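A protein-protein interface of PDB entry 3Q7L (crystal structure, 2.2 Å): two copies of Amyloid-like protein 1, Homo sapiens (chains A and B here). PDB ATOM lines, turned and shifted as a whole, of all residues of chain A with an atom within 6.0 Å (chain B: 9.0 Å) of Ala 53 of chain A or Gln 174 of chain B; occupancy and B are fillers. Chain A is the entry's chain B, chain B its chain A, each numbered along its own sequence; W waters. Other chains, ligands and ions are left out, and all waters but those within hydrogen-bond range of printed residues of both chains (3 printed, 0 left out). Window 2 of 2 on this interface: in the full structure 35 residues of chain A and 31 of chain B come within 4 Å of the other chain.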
ATOM      1  N   VAL A  48      -4.090  21.844  17.789  1.00  0.00           N
ATOM      2  CA  VAL A  48      -3.984  23.199  18.301  1.00  0.00           C
ATOM      3  C   VAL A  48      -2.655  23.377  19.013  1.00  0.00           C
ATOM      4  O   VAL A  48      -1.960  24.368  18.796  1.00  0.00           O
ATOM      5  CB  VAL A  48      -5.113  23.531  19.285  1.00  0.00           C
ATOM      6  CG1 VAL A  48      -4.885  24.921  19.912  1.00  0.00           C
ATOM      7  CG2 VAL A  48      -6.452  23.527  18.551  1.00  0.00           C
ATOM      8  N   MET A  49      -2.299  22.416  19.861  1.00  0.00           N
ATOM      9  CA  MET A  49      -1.047  22.486  20.603  1.00  0.00           C
ATOM     10  C   MET A  49       0.180  22.605  19.692  1.00  0.00           C
ATOM     11  O   MET A  49       1.138  23.303  20.021  1.00  0.00           O
ATOM     12  CB  MET A  49      -0.906  21.264  21.513  1.00  0.00           C
ATOM     13  CG  MET A  49      -1.903  21.232  22.661  1.00  0.00           C
ATOM     14  SD  MET A  49      -1.591  22.501  23.908  1.00  0.00           S
ATOM     15  CE  MET A  49      -3.022  22.226  24.991  1.00  0.00           C
ATOM     16  N   ARG A  50       0.149  21.917  18.559  1.00  0.00           N
ATOM     17  CA  ARG A  50       1.251  21.975  17.606  1.00  0.00           C
ATOM     18  C   ARG A  50       1.291  23.357  16.950  1.00  0.00           C
ATOM     19  O   ARG A  50       2.352  23.966  16.876  1.00  0.00           O
ATOM     20  CB  ARG A  50       1.113  20.881  16.545  1.00  0.00           C
ATOM     21  N   GLU A  51       0.140  23.847  16.483  1.00  0.00           N
ATOM     22  CA  GLU A  51       0.068  25.183  15.876  1.00  0.00           C
ATOM     23  C   GLU A  51       0.658  26.202  16.845  1.00  0.00           C
ATOM     24  O   GLU A  51       1.453  27.048  16.460  1.00  0.00           O
ATOM     25  CB  GLU A  51      -1.378  25.593  15.595  1.00  0.00           C
ATOM     26  CG  GLU A  51      -1.896  25.270  14.215  1.00  0.00           C
ATOM     27  CD  GLU A  51      -3.242  25.913  13.961  1.00  0.00           C
ATOM     28  OE1 GLU A  51      -3.320  27.165  13.943  1.00  0.00           O
ATOM     29  OE2 GLU A  51      -4.225  25.163  13.788  1.00  0.00           O
ATOM     30  N   TRP A  52       0.245  26.111  18.104  1.00  0.00           N
ATOM     31  CA  TRP A  52       0.709  27.011  19.144  1.00  0.00           C
ATOM     32  C   TRP A  52       2.227  26.878  19.333  1.00  0.00           C
ATOM     33  O   TRP A  52       2.904  27.856  19.629  1.00  0.00           O
ATOM     34  CB  TRP A  52      -0.031  26.692  20.447  1.00  0.00           C
ATOM     35  CG  TRP A  52       0.202  27.656  21.560  1.00  0.00           C
ATOM     36  CD1 TRP A  52       0.881  28.848  21.501  1.00  0.00           C
ATOM     37  CD2 TRP A  52      -0.240  27.524  22.917  1.00  0.00           C
ATOM     38  NE1 TRP A  52       0.899  29.448  22.736  1.00  0.00           N
ATOM     39  CE2 TRP A  52       0.229  28.647  23.624  1.00  0.00           C
ATOM     40  CE3 TRP A  52      -0.963  26.533  23.606  1.00  0.00           C
ATOM     41  CZ2 TRP A  52      -0.036  28.841  24.983  1.00  0.00           C
ATOM     42  CZ3 TRP A  52      -1.225  26.730  24.962  1.00  0.00           C
ATOM     43  CH2 TRP A  52      -0.748  27.867  25.636  1.00  0.00           C
ATOM     44  N   ALA A  53       2.751  25.662  19.171  1.00  0.00           N
ATOM     45  CA  ALA A  53       4.187  25.437  19.305  1.00  0.00           C
ATOM     46  C   ALA A  53       4.909  26.103  18.130  1.00  0.00           C
ATOM     47  O   ALA A  53       5.921  26.776  18.326  1.00  0.00           O
ATOM     48  CB  ALA A  53       4.502  23.937  19.338  1.00  0.00           C
ATOM     49  N   MET A  54       4.388  25.917  16.916  1.00  0.00           N
ATOM     50  CA  MET A  54       4.983  26.521  15.725  1.00  0.00           C
ATOM     51  C   MET A  54       4.946  28.048  15.833  1.00  0.00           C
ATOM     52  O   MET A  54       5.904  28.728  15.467  1.00  0.00           O
ATOM     53  CB  MET A  54       4.234  26.066  14.475  1.00  0.00           C
ATOM     54  N   ALA A  55       3.838  28.580  16.345  1.00  0.00           N
ATOM     55  CA  ALA A  55       3.701  30.023  16.509  1.00  0.00           C
ATOM     56  C   ALA A  55       4.764  30.561  17.475  1.00  0.00           C
ATOM     57  O   ALA A  55       5.375  31.599  17.207  1.00  0.00           O
ATOM     58  CB  ALA A  55       2.302  30.373  17.012  1.00  0.00           C
ATOM     59  N   ASP A  56       4.986  29.856  18.586  1.00  0.00           N
ATOM     60  CA  ASP A  56       5.983  30.274  19.572  1.00  0.00           C
ATOM     61  C   ASP A  56       7.399  30.324  18.994  1.00  0.00           C
ATOM     62  O   ASP A  56       8.198  31.180  19.370  1.00  0.00           O
ATOM     63  CB  ASP A  56       6.002  29.335  20.783  1.00  0.00           C
ATOM     64  CG  ASP A  56       4.801  29.508  21.688  1.00  0.00           C
ATOM     65  OD1 ASP A  56       4.157  30.574  21.654  1.00  0.00           O
ATOM     66  OD2 ASP A  56       4.511  28.574  22.455  1.00  0.00           O
ATOM     67  N   ASN A  57       7.710  29.387  18.107  1.00  0.00           N
ATOM     68  CA  ASN A  57       9.025  29.337  17.470  1.00  0.00           C
ATOM     69  C   ASN A  57       9.243  30.570  16.594  1.00  0.00           C
ATOM     70  O   ASN A  57      10.295  31.204  16.651  1.00  0.00           O
ATOM     71  CB  ASN A  57       9.153  28.073  16.607  1.00  0.00           C
ATOM     72  CG  ASN A  57       9.469  26.830  17.422  1.00  0.00           C
ATOM     73  OD1 ASN A  57      10.595  26.645  17.885  1.00  0.00           O
ATOM     74  ND2 ASN A  57       8.471  25.973  17.606  1.00  0.00           N
ATOM     75  N   GLN A  58       8.234  30.901  15.793  1.00  0.00           N
ATOM     76  CA  GLN A  58       8.266  32.046  14.879  1.00  0.00           C
ATOM     77  C   GLN A  58       8.194  33.395  15.562  1.00  0.00           C
ATOM     78  O   GLN A  58       8.813  34.353  15.122  1.00  0.00           O
ATOM     79  CB  GLN A  58       7.070  32.017  13.934  1.00  0.00           C
ATOM     80  CG  GLN A  58       7.111  31.028  12.826  1.00  0.00           C
ATOM     81  CD  GLN A  58       6.069  31.360  11.783  1.00  0.00           C
ATOM     82  OE1 GLN A  58       4.866  31.221  12.017  1.00  0.00           O
ATOM     83  NE2 GLN A  58       6.524  31.826  10.630  1.00  0.00           N
ATOM     84  N   GLU B 140       6.539   6.563  22.998  1.00  0.00           N
ATOM     85  CA  GLU B 140       6.441   8.020  23.145  1.00  0.00           C
ATOM     86  C   GLU B 140       5.006   8.491  22.881  1.00  0.00           C
ATOM     87  O   GLU B 140       4.488   9.389  23.550  1.00  0.00           O
ATOM     88  CB  GLU B 140       7.392   8.711  22.168  1.00  0.00           C
ATOM     89  CG  GLU B 140       8.863   8.582  22.523  1.00  0.00           C
ATOM     90  CD  GLU B 140       9.254   9.484  23.672  1.00  0.00           C
ATOM     91  OE1 GLU B 140      10.456   9.559  24.004  1.00  0.00           O
ATOM     92  OE2 GLU B 140       8.360  10.127  24.249  1.00  0.00           O
ATOM     93  N   GLN B 144       2.185  10.719  24.931  1.00  0.00           N
ATOM     94  CA  GLN B 144       1.556  11.861  24.275  1.00  0.00           C
ATOM     95  C   GLN B 144       0.034  11.705  24.420  1.00  0.00           C
ATOM     96  O   GLN B 144      -0.670  12.634  24.815  1.00  0.00           O
ATOM     97  CB  GLN B 144       1.946  11.880  22.791  1.00  0.00           C
ATOM     98  CG  GLN B 144       1.259  12.959  21.996  1.00  0.00           C
ATOM     99  CD  GLN B 144       1.433  12.760  20.506  1.00  0.00           C
ATOM    100  OE1 GLN B 144       1.229  11.661  19.989  1.00  0.00           O
ATOM    101  NE2 GLN B 144       1.806  13.823  19.808  1.00  0.00           N
ATOM    102  N   THR B 147      -1.071  12.349  27.920  1.00  0.00           N
ATOM    103  CA  THR B 147      -1.104  13.770  28.252  1.00  0.00           C
ATOM    104  C   THR B 147      -2.373  14.383  27.649  1.00  0.00           C
ATOM    105  O   THR B 147      -3.127  15.069  28.326  1.00  0.00           O
ATOM    106  CB  THR B 147       0.123  14.505  27.673  1.00  0.00           C
ATOM    107  OG1 THR B 147       1.324  13.888  28.150  1.00  0.00           O
ATOM    108  CG2 THR B 147       0.114  15.958  28.088  1.00  0.00           C
ATOM    109  N   ARG B 166      -3.426  24.262  30.624  1.00  0.00           N
ATOM    110  CA  ARG B 166      -2.981  24.643  29.285  1.00  0.00           C
ATOM    111  C   ARG B 166      -1.487  24.667  29.021  1.00  0.00           C
ATOM    112  O   ARG B 166      -0.990  23.868  28.223  1.00  0.00           O
ATOM    113  CB  ARG B 166      -3.590  25.982  28.887  1.00  0.00           C
ATOM    114  CG  ARG B 166      -5.015  25.840  28.406  1.00  0.00           C
ATOM    115  CD  ARG B 166      -5.643  27.183  28.150  1.00  0.00           C
ATOM    116  NE  ARG B 166      -7.073  27.144  28.428  1.00  0.00           N
ATOM    117  CZ  ARG B 166      -7.819  28.228  28.598  1.00  0.00           C
ATOM    118  NH1 ARG B 166      -7.259  29.429  28.516  1.00  0.00           N
ATOM    119  NH2 ARG B 166      -9.115  28.109  28.839  1.00  0.00           N
ATOM    120  N   PHE B 167      -0.772  25.577  29.680  1.00  0.00           N
ATOM    121  CA  PHE B 167       0.672  25.691  29.490  1.00  0.00           C
ATOM    122  C   PHE B 167       1.424  24.400  29.760  1.00  0.00           C
ATOM    123  O   PHE B 167       2.273  24.000  28.953  1.00  0.00           O
ATOM    124  CB  PHE B 167       1.239  26.823  30.352  1.00  0.00           C
ATOM    125  CG  PHE B 167       1.219  28.159  29.675  1.00  0.00           C
ATOM    126  CD1 PHE B 167       1.980  28.377  28.529  1.00  0.00           C
ATOM    127  CD2 PHE B 167       0.436  29.202  30.171  1.00  0.00           C
ATOM    128  CE1 PHE B 167       1.960  29.612  27.884  1.00  0.00           C
ATOM    129  CE2 PHE B 167       0.407  30.445  29.533  1.00  0.00           C
ATOM    130  CZ  PHE B 167       1.172  30.650  28.388  1.00  0.00           C
ATOM    131  N   GLN B 168       1.123  23.747  30.883  1.00  0.00           N
ATOM    132  CA  GLN B 168       1.780  22.486  31.219  1.00  0.00           C
ATOM    133  C   GLN B 168       1.639  21.478  30.081  1.00  0.00           C
ATOM    134  O   GLN B 168       2.618  20.862  29.670  1.00  0.00           O
ATOM    135  CB  GLN B 168       1.174  21.856  32.473  1.00  0.00           C
ATOM    136  CG  GLN B 168       1.301  22.666  33.732  1.00  0.00           C
ATOM    137  CD  GLN B 168       1.107  21.808  34.966  1.00  0.00           C
ATOM    138  OE1 GLN B 168       2.006  21.062  35.364  1.00  0.00           O
ATOM    139  NE2 GLN B 168      -0.075  21.892  35.569  1.00  0.00           N
ATOM    140  N   VAL B 169       0.415  21.299  29.593  1.00  0.00           N
ATOM    141  CA  VAL B 169       0.164  20.352  28.511  1.00  0.00           C
ATOM    142  C   VAL B 169       0.990  20.763  27.296  1.00  0.00           C
ATOM    143  O   VAL B 169       1.697  19.951  26.698  1.00  0.00           O
ATOM    144  CB  VAL B 169      -1.329  20.329  28.105  1.00  0.00           C
ATOM    145  CG1 VAL B 169      -1.542  19.343  26.966  1.00  0.00           C
ATOM    146  CG2 VAL B 169      -2.194  19.953  29.300  1.00  0.00           C
ATOM    147  N   HIS B 170       0.883  22.037  26.945  1.00  0.00           N
ATOM    148  CA  HIS B 170       1.604  22.612  25.816  1.00  0.00           C
ATOM    149  C   HIS B 170       3.100  22.319  25.933  1.00  0.00           C
ATOM    150  O   HIS B 170       3.719  21.788  25.013  1.00  0.00           O
ATOM    151  CB  HIS B 170       1.366  24.122  25.809  1.00  0.00           C
ATOM    152  CG  HIS B 170       2.086  24.851  24.722  1.00  0.00           C
ATOM    153  ND1 HIS B 170       2.035  24.466  23.401  1.00  0.00           N
ATOM    154  CD2 HIS B 170       2.827  25.988  24.753  1.00  0.00           C
ATOM    155  CE1 HIS B 170       2.708  25.329  22.662  1.00  0.00           C
ATOM    156  NE2 HIS B 170       3.197  26.263  23.462  1.00  0.00           N
ATOM    157  N   THR B 171       3.667  22.662  27.086  1.00  0.00           N
ATOM    158  CA  THR B 171       5.081  22.453  27.340  1.00  0.00           C
ATOM    159  C   THR B 171       5.464  20.977  27.250  1.00  0.00           C
ATOM    160  O   THR B 171       6.425  20.626  26.563  1.00  0.00           O
ATOM    161  CB  THR B 171       5.466  23.005  28.731  1.00  0.00           C
ATOM    162  OG1 THR B 171       5.204  24.418  28.775  1.00  0.00           O
ATOM    163  CG2 THR B 171       6.934  22.752  29.015  1.00  0.00           C
ATOM    164  N   HIS B 172       4.703  20.120  27.928  1.00  0.00           N
ATOM    165  CA  HIS B 172       4.969  18.679  27.951  1.00  0.00           C
ATOM    166  C   HIS B 172       4.944  18.029  26.562  1.00  0.00           C
ATOM    167  O   HIS B 172       5.843  17.259  26.217  1.00  0.00           O
ATOM    168  CB  HIS B 172       3.968  17.989  28.906  1.00  0.00           C
ATOM    169  CG  HIS B 172       4.275  16.545  29.188  1.00  0.00           C
ATOM    170  ND1 HIS B 172       3.542  15.795  30.092  1.00  0.00           N
ATOM    171  CD2 HIS B 172       5.199  15.699  28.673  1.00  0.00           C
ATOM    172  CE1 HIS B 172       4.003  14.555  30.110  1.00  0.00           C
ATOM    173  NE2 HIS B 172       5.004  14.471  29.261  1.00  0.00           N
ATOM    174  N   LEU B 173       3.933  18.332  25.751  1.00  0.00           N
ATOM    175  CA  LEU B 173       3.866  17.742  24.413  1.00  0.00           C
ATOM    176  C   LEU B 173       5.088  18.160  23.595  1.00  0.00           C
ATOM    177  O   LEU B 173       5.578  17.391  22.769  1.00  0.00           O
ATOM    178  CB  LEU B 173       2.596  18.175  23.687  1.00  0.00           C
ATOM    179  CG  LEU B 173       1.295  17.669  24.310  1.00  0.00           C
ATOM    180  CD1 LEU B 173       0.116  18.367  23.642  1.00  0.00           C
ATOM    181  CD2 LEU B 173       1.203  16.167  24.139  1.00  0.00           C
ATOM    182  N   GLN B 174       5.577  19.378  23.814  1.00  0.00           N
ATOM    183  CA  GLN B 174       6.754  19.827  23.087  1.00  0.00           C
ATOM    184  C   GLN B 174       7.966  19.058  23.586  1.00  0.00           C
ATOM    185  O   GLN B 174       8.844  18.694  22.802  1.00  0.00           O
ATOM    186  CB  GLN B 174       6.967  21.319  23.276  1.00  0.00           C
ATOM    187  CG  GLN B 174       6.154  22.152  22.334  1.00  0.00           C
ATOM    188  CD  GLN B 174       6.416  23.616  22.539  1.00  0.00           C
ATOM    189  OE1 GLN B 174       5.939  24.218  23.507  1.00  0.00           O
ATOM    190  NE2 GLN B 174       7.202  24.202  21.640  1.00  0.00           N
ATOM    191  N   VAL B 175       8.009  18.805  24.893  1.00  0.00           N
ATOM    192  CA  VAL B 175       9.109  18.034  25.452  1.00  0.00           C
ATOM    193  C   VAL B 175       9.139  16.665  24.772  1.00  0.00           C
ATOM    194  O   VAL B 175      10.196  16.202  24.365  1.00  0.00           O
ATOM    195  CB  VAL B 175       8.959  17.818  26.970  1.00  0.00           C
ATOM    196  CG1 VAL B 175       9.968  16.764  27.443  1.00  0.00           C
ATOM    197  CG2 VAL B 175       9.184  19.127  27.703  1.00  0.00           C
ATOM    198  N   ILE B 176       7.980  16.025  24.641  1.00  0.00           N
ATOM    199  CA  ILE B 176       7.908  14.718  23.991  1.00  0.00           C
ATOM    200  C   ILE B 176       8.389  14.746  22.541  1.00  0.00           C
ATOM    201  O   ILE B 176       9.187  13.906  22.127  1.00  0.00           O
ATOM    202  CB  ILE B 176       6.454  14.160  23.990  1.00  0.00           C
ATOM    203  CG1 ILE B 176       5.953  13.991  25.430  1.00  0.00           C
ATOM    204  CG2 ILE B 176       6.406  12.815  23.269  1.00  0.00           C
ATOM    205  CD1 ILE B 176       4.503  13.515  25.540  1.00  0.00           C
ATOM    206  N   GLU B 177       7.886  15.704  21.764  1.00  0.00           N
ATOM    207  CA  GLU B 177       8.245  15.814  20.354  1.00  0.00           C
ATOM    208  C   GLU B 177       9.742  15.997  20.173  1.00  0.00           C
ATOM    209  O   GLU B 177      10.338  15.404  19.283  1.00  0.00           O
ATOM    210  CB  GLU B 177       7.492  16.976  19.702  1.00  0.00           C
ATOM    211  N   GLU B 178      10.341  16.828  21.017  1.00  0.00           N
ATOM    212  CA  GLU B 178      11.774  17.062  20.945  1.00  0.00           C
ATOM    213  C   GLU B 178      12.516  15.754  21.242  1.00  0.00           C
ATOM    214  O   GLU B 178      13.429  15.380  20.504  1.00  0.00           O
ATOM    215  CB  GLU B 178      12.183  18.163  21.931  1.00  0.00           C
ATOM    216  CG  GLU B 178      12.822  19.380  21.259  1.00  0.00           C
ATOM    217  CD  GLU B 178      14.038  19.010  20.408  1.00  0.00           C
ATOM    218  OE1 GLU B 178      15.092  18.649  20.980  1.00  0.00           O
ATOM    219  OE2 GLU B 178      13.932  19.062  19.161  1.00  0.00           O
ATOM    220  N   ARG B 179      12.116  15.048  22.305  1.00  0.00           N
ATOM    221  CA  ARG B 179      12.766  13.774  22.654  1.00  0.00           C
ATOM    222  C   ARG B 179      12.795  12.852  21.451  1.00  0.00           C
ATOM    223  O   ARG B 179      13.833  12.296  21.110  1.00  0.00           O
ATOM    224  CB  ARG B 179      12.025  13.040  23.783  1.00  0.00           C
ATOM    225  CG  ARG B 179      12.677  13.089  25.159  1.00  0.00           C
ATOM    226  CD  ARG B 179      12.322  11.835  25.982  1.00  0.00           C
ATOM    227  NE  ARG B 179      10.893  11.505  25.945  1.00  0.00           N
ATOM    228  CZ  ARG B 179      10.000  11.837  26.875  1.00  0.00           C
ATOM    229  NH1 ARG B 179      10.374  12.515  27.950  1.00  0.00           N
ATOM    230  NH2 ARG B 179       8.722  11.483  26.724  1.00  0.00           N
ATOM    231  N   VAL B 180      11.641  12.678  20.813  1.00  0.00           N
ATOM    232  CA  VAL B 180      11.545  11.815  19.643  1.00  0.00           C
ATOM    233  C   VAL B 180      12.525  12.244  18.554  1.00  0.00           C
ATOM    234  O   VAL B 180      13.152  11.399  17.913  1.00  0.00           O
ATOM    235  CB  VAL B 180      10.120  11.817  19.059  1.00  0.00           C
ATOM    236  CG1 VAL B 180      10.099  11.038  17.753  1.00  0.00           C
ATOM    237  CG2 VAL B 180       9.136  11.200  20.065  1.00  0.00           C
ATOM    238  N   ASN B 181      12.660  13.554  18.344  1.00  0.00           N
ATOM    239  CA  ASN B 181      13.585  14.044  17.326  1.00  0.00           C
ATOM    240  C   ASN B 181      15.019  13.698  17.729  1.00  0.00           C
ATOM    241  O   ASN B 181      15.784  13.168  16.929  1.00  0.00           O
ATOM    242  CB  ASN B 181      13.428  15.558  17.119  1.00  0.00           C
ATOM    243  CG  ASN B 181      12.119  15.920  16.430  1.00  0.00           C
ATOM    244  OD1 ASN B 181      11.568  15.127  15.660  1.00  0.00           O
ATOM    245  ND2 ASN B 181      11.625  17.127  16.689  1.00  0.00           N
ATOM    246  N   GLN B 182      15.376  13.991  18.976  1.00  0.00           N
ATOM    247  CA  GLN B 182      16.708  13.673  19.472  1.00  0.00           C
ATOM    248  C   GLN B 182      17.043  12.189  19.317  1.00  0.00           C
ATOM    249  O   GLN B 182      18.183  11.836  19.006  1.00  0.00           O
ATOM    250  CB  GLN B 182      16.837  14.056  20.948  1.00  0.00           C
ATOM    251  CG  GLN B 182      17.136  15.515  21.181  1.00  0.00           C
ATOM    252  CD  GLN B 182      18.390  15.948  20.449  1.00  0.00           C
ATOM    253  OE1 GLN B 182      19.437  15.303  20.556  1.00  0.00           O
ATOM    254  NE2 GLN B 182      18.294  17.037  19.701  1.00  0.00           N
HETATM  255  O   HOH W   1       8.408  23.425  19.496  1.00  0.00           O
HETATM  256  O   HOH W   2       6.440  27.119  23.493  1.00  0.00           O
HETATM  257  O   HOH W   3       2.441  21.894  22.494  1.00  0.00           O
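A ring nitrogen (NE2) of His 170 of chain B lies within hydrogen-bond range of the side-chain carboxylate (OD2) of Asp 56 of chain A (2.8 Å).
The side-chain amide oxygen (OE1) of Gln 174 of chain B lies within hydrogen-bond range of a ring nitrogen (NE2) of His 170 of chain B (3.4 Å).
The backbone carbonyl oxygen (O) of Phe 167 of chain B sits at hydrogen-bond distance from the side-chain hydroxyl (OG1) of Thr 171 of chain B, at 3.0 Å.
The backbone carbonyl oxygen (O) of Ala 53 of chain A lies within hydrogen-bond range of the side-chain amide nitrogen (ND2) of Asn 57 of chain A (2.8 Å).
Among the printed residues, merely in contact across the chains: Ala 53 of chain A with His 170 of chain B (3.5 Å), Ala 53 of chain A with Gln 174 of chain B (3.6 Å), Trp 52 of chain A with His 170 of chain B (3.6 Å), Trp 52 of chain A with Phe 167 of chain B (3.6 Å), Met 49 of chain A with Leu 173 of chain B (3.6 Å), Met 49 of chain A with His 170 of chain B (3.7 Å) and Met 49 of chain A with Val 169 of chain B (3.8 Å).
Gln 174 of chain B touches just one residue of chain A: Ala 53.
No residue of chain B comes within 4 Å of Met 54 of chain A.
Of the printed residues of chain B, Asp 56 of chain A touches His 170 (2.8 Å).
Printed residues of chain A within 4 Å of Leu 173 of chain B: Met 49.
Printed residues of chain A within 4 Å of His 170 of chain B: Met 49 (3.7 Å), Trp 52 (3.6 Å), Ala 53 (3.5 Å) and Asp 56 (2.8 Å).
Arg 179 of chain B touches none of the printed residues of chain A.
The nearest residue of chain B that does not touch Ala 53 of chain A is Leu 173 of chain B (7.2 Å).
Hydrophobic or aromatic side chains of chain A that line the printed part of chain B: Met 49, Trp 52 and Ala 53.
Of the 20 printed residues of chain B, 5 touch a printed residue of chain A.
Printed residues of chain B that touch a printed residue of chain A: Phe 167, Val 169, His 170, Leu 173 and Gln 174.
Among the printed residues, 8 pairs touch across the chains.
Among the printed residues, no Asp or Glu carboxylate lies within 4 Å of a Lys or Arg side-chain nitrogen of the other chain.
No position is printed for both chains.
Of the 8 pairs that touch across the chains among the printed residues, none has its exchanged pair printed and touching as well.
Water W1 bridges the side-chain amide nitrogen (NE2) of Gln 174 of chain B (2.6 Å) and the side-chain amide nitrogen (ND2) of Asn 57 of chain A (3.2 Å).
Water W2 lies within hydrogen-bond range of the side-chain carboxylate of Asp 56 of chain A (2.6 Å), the side-chain amide oxygen of Gln 174 of chain B (2.9 Å) and a ring nitrogen (NE2) of His 170 of chain B (3.4 Å).
Water W3 lies within hydrogen-bond range of ND1 of His 170 of chain B (2.8 Å) and O of Met 49 of chain A (3.1 Å).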
